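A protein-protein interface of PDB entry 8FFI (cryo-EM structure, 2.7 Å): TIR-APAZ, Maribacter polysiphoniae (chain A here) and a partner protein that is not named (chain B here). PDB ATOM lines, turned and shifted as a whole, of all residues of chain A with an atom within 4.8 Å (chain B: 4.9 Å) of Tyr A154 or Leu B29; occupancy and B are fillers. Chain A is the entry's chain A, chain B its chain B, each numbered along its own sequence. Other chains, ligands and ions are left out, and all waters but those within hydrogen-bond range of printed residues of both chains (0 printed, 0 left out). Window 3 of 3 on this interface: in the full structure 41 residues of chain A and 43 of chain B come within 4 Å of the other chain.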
ATOM      1  N   ARG A  19       9.216 -26.945  12.510  1.00  0.00           N
ATOM      2  CA  ARG A  19      10.653 -27.157  12.654  1.00  0.00           C
ATOM      3  C   ARG A  19      11.437 -26.202  11.766  1.00  0.00           C
ATOM      4  O   ARG A  19      12.404 -25.574  12.212  1.00  0.00           O
ATOM      5  CB  ARG A  19      11.004 -28.607  12.325  1.00  0.00           C
ATOM      6  CG  ARG A  19      12.485 -28.932  12.419  1.00  0.00           C
ATOM      7  CD  ARG A  19      12.731 -30.415  12.198  1.00  0.00           C
ATOM      8  NE  ARG A  19      12.516 -30.818  10.814  1.00  0.00           N
ATOM      9  CZ  ARG A  19      13.484 -31.001   9.927  1.00  0.00           C
ATOM     10  NH1 ARG A  19      14.758 -30.840  10.250  1.00  0.00           N
ATOM     11  NH2 ARG A  19      13.169 -31.359   8.685  1.00  0.00           N
ATOM     12  N   LEU A  23      13.771 -23.326  13.494  1.00  0.00           N
ATOM     13  CA  LEU A  23      15.215 -23.377  13.303  1.00  0.00           C
ATOM     14  C   LEU A  23      15.718 -22.157  12.539  1.00  0.00           C
ATOM     15  O   LEU A  23      16.791 -21.631  12.849  1.00  0.00           O
ATOM     16  CB  LEU A  23      15.601 -24.678  12.600  1.00  0.00           C
ATOM     17  CG  LEU A  23      15.455 -25.905  13.506  1.00  0.00           C
ATOM     18  CD1 LEU A  23      16.110 -27.134  12.911  1.00  0.00           C
ATOM     19  CD2 LEU A  23      16.038 -25.610  14.877  1.00  0.00           C
ATOM     20  N   LYS A  24      14.948 -21.667  11.562  1.00  0.00           N
ATOM     21  CA  LYS A  24      15.344 -20.437  10.882  1.00  0.00           C
ATOM     22  C   LYS A  24      15.376 -19.256  11.848  1.00  0.00           C
ATOM     23  O   LYS A  24      16.327 -18.466  11.845  1.00  0.00           O
ATOM     24  CB  LYS A  24      14.399 -20.156   9.713  1.00  0.00           C
ATOM     25  CG  LYS A  24      14.683 -20.977   8.461  1.00  0.00           C
ATOM     26  CD  LYS A  24      15.917 -20.477   7.728  1.00  0.00           C
ATOM     27  CE  LYS A  24      16.094 -21.185   6.393  1.00  0.00           C
ATOM     28  NZ  LYS A  24      17.083 -20.494   5.523  1.00  0.00           N
ATOM     29  N   SER A 150      20.833 -22.985  15.870  1.00  0.00           N
ATOM     30  CA  SER A 150      19.907 -23.847  15.146  1.00  0.00           C
ATOM     31  C   SER A 150      20.566 -25.168  14.770  1.00  0.00           C
ATOM     32  O   SER A 150      19.932 -26.226  14.835  1.00  0.00           O
ATOM     33  CB  SER A 150      19.388 -23.127  13.903  1.00  0.00           C
ATOM     34  OG  SER A 150      20.445 -22.482  13.216  1.00  0.00           O
ATOM     35  N   ASN A 151      21.840 -25.123  14.371  1.00  0.00           N
ATOM     36  CA  ASN A 151      22.579 -26.345  14.070  1.00  0.00           C
ATOM     37  C   ASN A 151      22.613 -27.276  15.276  1.00  0.00           C
ATOM     38  O   ASN A 151      22.290 -28.466  15.171  1.00  0.00           O
ATOM     39  CB  ASN A 151      23.998 -25.992  13.622  1.00  0.00           C
ATOM     40  CG  ASN A 151      24.568 -26.989  12.637  1.00  0.00           C
ATOM     41  OD1 ASN A 151      24.121 -28.132  12.562  1.00  0.00           O
ATOM     42  ND2 ASN A 151      25.564 -26.560  11.874  1.00  0.00           N
ATOM     43  N   LEU A 152      23.002 -26.742  16.436  1.00  0.00           N
ATOM     44  CA  LEU A 152      23.097 -27.557  17.641  1.00  0.00           C
ATOM     45  C   LEU A 152      21.737 -28.104  18.053  1.00  0.00           C
ATOM     46  O   LEU A 152      21.626 -29.269  18.451  1.00  0.00           O
ATOM     47  CB  LEU A 152      23.716 -26.740  18.775  1.00  0.00           C
ATOM     48  CG  LEU A 152      24.118 -27.502  20.039  1.00  0.00           C
ATOM     49  CD1 LEU A 152      25.456 -27.001  20.549  1.00  0.00           C
ATOM     50  CD2 LEU A 152      23.050 -27.364  21.115  1.00  0.00           C
ATOM     51  N   LEU A 153      20.690 -27.280  17.973  1.00  0.00           N
ATOM     52  CA  LEU A 153      19.370 -27.748  18.380  1.00  0.00           C
ATOM     53  C   LEU A 153      18.863 -28.831  17.434  1.00  0.00           C
ATOM     54  O   LEU A 153      18.246 -29.810  17.871  1.00  0.00           O
ATOM     55  CB  LEU A 153      18.394 -26.571  18.451  1.00  0.00           C
ATOM     56  CG  LEU A 153      16.994 -26.798  19.037  1.00  0.00           C
ATOM     57  CD1 LEU A 153      16.470 -25.496  19.612  1.00  0.00           C
ATOM     58  CD2 LEU A 153      16.003 -27.367  18.030  1.00  0.00           C
ATOM     59  N   TYR A 154      19.119 -28.676  16.133  1.00  0.00           N
ATOM     60  CA  TYR A 154      18.746 -29.703  15.166  1.00  0.00           C
ATOM     61  C   TYR A 154      19.492 -31.002  15.435  1.00  0.00           C
ATOM     62  O   TYR A 154      18.921 -32.093  15.336  1.00  0.00           O
ATOM     63  CB  TYR A 154      19.020 -29.196  13.748  1.00  0.00           C
ATOM     64  CG  TYR A 154      19.032 -30.266  12.681  1.00  0.00           C
ATOM     65  CD1 TYR A 154      17.880 -30.967  12.356  1.00  0.00           C
ATOM     66  CD2 TYR A 154      20.199 -30.567  11.991  1.00  0.00           C
ATOM     67  CE1 TYR A 154      17.891 -31.942  11.379  1.00  0.00           C
ATOM     68  CE2 TYR A 154      20.219 -31.538  11.012  1.00  0.00           C
ATOM     69  CZ  TYR A 154      19.063 -32.223  10.712  1.00  0.00           C
ATOM     70  OH  TYR A 154      19.078 -33.192   9.737  1.00  0.00           O
ATOM     71  N   GLN A 155      20.780 -30.903  15.773  1.00  0.00           N
ATOM     72  CA  GLN A 155      21.553 -32.101  16.082  1.00  0.00           C
ATOM     73  C   GLN A 155      21.035 -32.790  17.339  1.00  0.00           C
ATOM     74  O   GLN A 155      20.951 -34.022  17.391  1.00  0.00           O
ATOM     75  CB  GLN A 155      23.031 -31.750  16.239  1.00  0.00           C
ATOM     76  CG  GLN A 155      23.780 -31.587  14.930  1.00  0.00           C
ATOM     77  CD  GLN A 155      25.049 -30.775  15.087  1.00  0.00           C
ATOM     78  OE1 GLN A 155      25.520 -30.552  16.202  1.00  0.00           O
ATOM     79  NE2 GLN A 155      25.609 -30.326  13.970  1.00  0.00           N
ATOM     80  N   GLN A 156      20.686 -32.013  18.367  1.00  0.00           N
ATOM     81  CA  GLN A 156      20.364 -32.597  19.663  1.00  0.00           C
ATOM     82  C   GLN A 156      18.904 -33.004  19.807  1.00  0.00           C
ATOM     83  O   GLN A 156      18.588 -33.793  20.701  1.00  0.00           O
ATOM     84  CB  GLN A 156      20.730 -31.624  20.786  1.00  0.00           C
ATOM     85  CG  GLN A 156      19.586 -30.738  21.241  1.00  0.00           C
ATOM     86  CD  GLN A 156      20.018 -29.711  22.265  1.00  0.00           C
ATOM     87  OE1 GLN A 156      21.193 -29.630  22.622  1.00  0.00           O
ATOM     88  NE2 GLN A 156      19.066 -28.919  22.746  1.00  0.00           N
ATOM     89  N   ILE A 157      18.010 -32.495  18.966  1.00  0.00           N
ATOM     90  CA  ILE A 157      16.587 -32.807  19.071  1.00  0.00           C
ATOM     91  C   ILE A 157      16.136 -33.757  17.971  1.00  0.00           C
ATOM     92  O   ILE A 157      15.517 -34.785  18.244  1.00  0.00           O
ATOM     93  CB  ILE A 157      15.747 -31.510  19.062  1.00  0.00           C
ATOM     94  CG1 ILE A 157      16.125 -30.611  20.238  1.00  0.00           C
ATOM     95  CG2 ILE A 157      14.273 -31.846  19.109  1.00  0.00           C
ATOM     96  CD1 ILE A 157      15.708 -31.160  21.580  1.00  0.00           C
ATOM     97  N   PHE A 158      16.435 -33.427  16.717  1.00  0.00           N
ATOM     98  CA  PHE A 158      15.913 -34.169  15.578  1.00  0.00           C
ATOM     99  C   PHE A 158      16.869 -35.233  15.059  1.00  0.00           C
ATOM    100  O   PHE A 158      16.466 -36.052  14.226  1.00  0.00           O
ATOM    101  CB  PHE A 158      15.551 -33.193  14.454  1.00  0.00           C
ATOM    102  CG  PHE A 158      14.756 -32.007  14.926  1.00  0.00           C
ATOM    103  CD1 PHE A 158      13.411 -32.134  15.224  1.00  0.00           C
ATOM    104  CD2 PHE A 158      15.358 -30.773  15.096  1.00  0.00           C
ATOM    105  CE1 PHE A 158      12.677 -31.048  15.668  1.00  0.00           C
ATOM    106  CE2 PHE A 158      14.630 -29.686  15.540  1.00  0.00           C
ATOM    107  CZ  PHE A 158      13.288 -29.824  15.826  1.00  0.00           C
ATOM    108  N   LEU A 159      18.116 -35.250  15.531  1.00  0.00           N
ATOM    109  CA  LEU A 159      19.070 -36.302  15.214  1.00  0.00           C
ATOM    110  C   LEU A 159      19.380 -37.169  16.428  1.00  0.00           C
ATOM    111  O   LEU A 159      20.385 -37.886  16.437  1.00  0.00           O
ATOM    112  CB  LEU A 159      20.359 -35.701  14.651  1.00  0.00           C
ATOM    113  CG  LEU A 159      20.260 -34.960  13.319  1.00  0.00           C
ATOM    114  CD1 LEU A 159      21.603 -34.353  12.955  1.00  0.00           C
ATOM    115  CD2 LEU A 159      19.774 -35.892  12.225  1.00  0.00           C
ATOM    116  N   CYS B  20      27.137 -30.238   7.780  1.00  0.00           N
ATOM    117  CA  CYS B  20      26.055 -31.205   7.869  1.00  0.00           C
ATOM    118  C   CYS B  20      26.446 -32.439   7.072  1.00  0.00           C
ATOM    119  O   CYS B  20      27.306 -32.383   6.192  1.00  0.00           O
ATOM    120  CB  CYS B  20      24.735 -30.620   7.354  1.00  0.00           C
ATOM    121  SG  CYS B  20      23.264 -31.579   7.771  1.00  0.00           S
ATOM    122  N   ASP B  25      19.139 -31.357   4.034  1.00  0.00           N
ATOM    123  CA  ASP B  25      18.974 -30.717   5.334  1.00  0.00           C
ATOM    124  C   ASP B  25      19.791 -29.437   5.431  1.00  0.00           C
ATOM    125  O   ASP B  25      19.303 -28.417   5.929  1.00  0.00           O
ATOM    126  CB  ASP B  25      19.363 -31.685   6.448  1.00  0.00           C
ATOM    127  CG  ASP B  25      18.253 -32.655   6.786  1.00  0.00           C
ATOM    128  OD1 ASP B  25      17.118 -32.449   6.309  1.00  0.00           O
ATOM    129  OD2 ASP B  25      18.514 -33.619   7.532  1.00  0.00           O
ATOM    130  N   GLY B  26      21.037 -29.467   4.957  1.00  0.00           N
ATOM    131  CA  GLY B  26      21.867 -28.279   5.020  1.00  0.00           C
ATOM    132  C   GLY B  26      21.386 -27.168   4.111  1.00  0.00           C
ATOM    133  O   GLY B  26      21.599 -25.988   4.403  1.00  0.00           O
ATOM    134  N   LEU B  27      20.737 -27.520   3.001  1.00  0.00           N
ATOM    135  CA  LEU B  27      20.176 -26.507   2.117  1.00  0.00           C
ATOM    136  C   LEU B  27      18.894 -25.917   2.690  1.00  0.00           C
ATOM    137  O   LEU B  27      18.638 -24.719   2.535  1.00  0.00           O
ATOM    138  CB  LEU B  27      19.917 -27.102   0.732  1.00  0.00           C
ATOM    139  CG  LEU B  27      21.109 -27.110  -0.226  1.00  0.00           C
ATOM    140  CD1 LEU B  27      20.769 -27.871  -1.494  1.00  0.00           C
ATOM    141  CD2 LEU B  27      21.552 -25.690  -0.543  1.00  0.00           C
ATOM    142  N   ALA B  28      18.078 -26.739   3.355  1.00  0.00           N
ATOM    143  CA  ALA B  28      16.860 -26.217   3.963  1.00  0.00           C
ATOM    144  C   ALA B  28      17.156 -25.410   5.221  1.00  0.00           C
ATOM    145  O   ALA B  28      16.389 -24.505   5.568  1.00  0.00           O
ATOM    146  CB  ALA B  28      15.897 -27.361   4.277  1.00  0.00           C
ATOM    147  N   LEU B  29      18.251 -25.716   5.915  1.00  0.00           N
ATOM    148  CA  LEU B  29      18.598 -25.024   7.151  1.00  0.00           C
ATOM    149  C   LEU B  29      19.410 -23.755   6.915  1.00  0.00           C
ATOM    150  O   LEU B  29      19.131 -22.718   7.523  1.00  0.00           O
ATOM    151  CB  LEU B  29      19.374 -25.964   8.079  1.00  0.00           C
ATOM    152  CG  LEU B  29      18.601 -27.095   8.754  1.00  0.00           C
ATOM    153  CD1 LEU B  29      19.545 -28.180   9.238  1.00  0.00           C
ATOM    154  CD2 LEU B  29      17.797 -26.540   9.902  1.00  0.00           C
ATOM    155  N   PHE B  30      20.419 -23.818   6.049  1.00  0.00           N
ATOM    156  CA  PHE B  30      21.417 -22.760   5.961  1.00  0.00           C
ATOM    157  C   PHE B  30      21.437 -22.056   4.614  1.00  0.00           C
ATOM    158  O   PHE B  30      21.444 -20.819   4.570  1.00  0.00           O
ATOM    159  CB  PHE B  30      22.806 -23.336   6.272  1.00  0.00           C
ATOM    160  CG  PHE B  30      22.881 -24.061   7.587  1.00  0.00           C
ATOM    161  CD1 PHE B  30      22.508 -23.432   8.763  1.00  0.00           C
ATOM    162  CD2 PHE B  30      23.315 -25.375   7.643  1.00  0.00           C
ATOM    163  CE1 PHE B  30      22.573 -24.099   9.972  1.00  0.00           C
ATOM    164  CE2 PHE B  30      23.383 -26.046   8.848  1.00  0.00           C
ATOM    165  CZ  PHE B  30      23.012 -25.407  10.013  1.00  0.00           C
ATOM    166  N   GLY B  31      21.458 -22.798   3.510  1.00  0.00           N
ATOM    167  CA  GLY B  31      21.523 -22.204   2.195  1.00  0.00           C
ATOM    168  C   GLY B  31      22.860 -22.418   1.513  1.00  0.00           C
ATOM    169  O   GLY B  31      23.803 -22.958   2.096  1.00  0.00           O
ATOM    170  N   LYS B 428      20.836 -42.282   9.617  1.00  0.00           N
ATOM    171  CA  LYS B 428      20.292 -40.928   9.648  1.00  0.00           C
ATOM    172  C   LYS B 428      18.918 -40.860   8.991  1.00  0.00           C
ATOM    173  O   LYS B 428      18.013 -40.187   9.497  1.00  0.00           O
ATOM    174  CB  LYS B 428      21.269 -39.967   8.968  1.00  0.00           C
ATOM    175  CG  LYS B 428      20.936 -38.495   9.138  1.00  0.00           C
ATOM    176  CD  LYS B 428      20.208 -37.950   7.922  1.00  0.00           C
ATOM    177  CE  LYS B 428      19.729 -36.535   8.158  1.00  0.00           C
ATOM    178  NZ  LYS B 428      18.757 -36.109   7.117  1.00  0.00           N
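The side-chain hydroxyl (OH) of Tyr A154 lies close to the side-chain carboxylate (OD2) of Asp B25.
The side-chain amino group (NZ) of Lys B428 lies within salt-bridge range of the side-chain carboxylate (OD2) of Asp B25, at 2.5 Å.
OD1 of Asn A151 lies within hydrogen-bond range of NE2 of Gln A155, at 3.0 Å.
The backbone carbonyl oxygen (O) of Tyr A154 is in hydrogen-bond range of the backbone NH (N) of Leu A159, 3.3 Å away.
Among the printed residues, merely in contact across the chains: Leu A23 with Leu B29 (3.5 Å), Lys A24 with Ala B28 (3.4 Å), Lys A24 with Leu B29 (3.6 Å), Asn A151 with Phe B30 (3.4 Å), Tyr A154 with Leu B29 (3.7 Å) and Tyr A154 with Lys B428 (3.8 Å).
Leu A152 touches none of the printed residues of chain B.
Cys B20 touches none of the printed residues of chain A.
Of the printed residues of chain A, Asp B25 touches Tyr A154.
Of chain A, only Leu A23, Lys A24 and Tyr A154 come within 4 Å of Leu B29.
Of the printed residues of chain A, Phe B30 touches Asn A151 (3.4 Å).
The nearest residue of chain B that does not touch Tyr A154 is Cys B20 (4.4 Å).
Printed residues of chain A that touch a printed residue of chain B: Leu A23, Lys A24, Asn A151 and Tyr A154.
Hydrophobic or aromatic side chains of chain A within 4 Å of the printed part of chain B: Leu A23 and Tyr A154.
Of the 9 printed residues of chain B, 5 touch a printed residue of chain A.
Hydrophobic or aromatic side chains of chain B within 4 Å of the printed part of chain A: Leu B29 and Phe B30.
Among the printed residues, no Asp or Glu carboxylate lies within 4 Å of a Lys or Arg side-chain nitrogen of the other chain.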
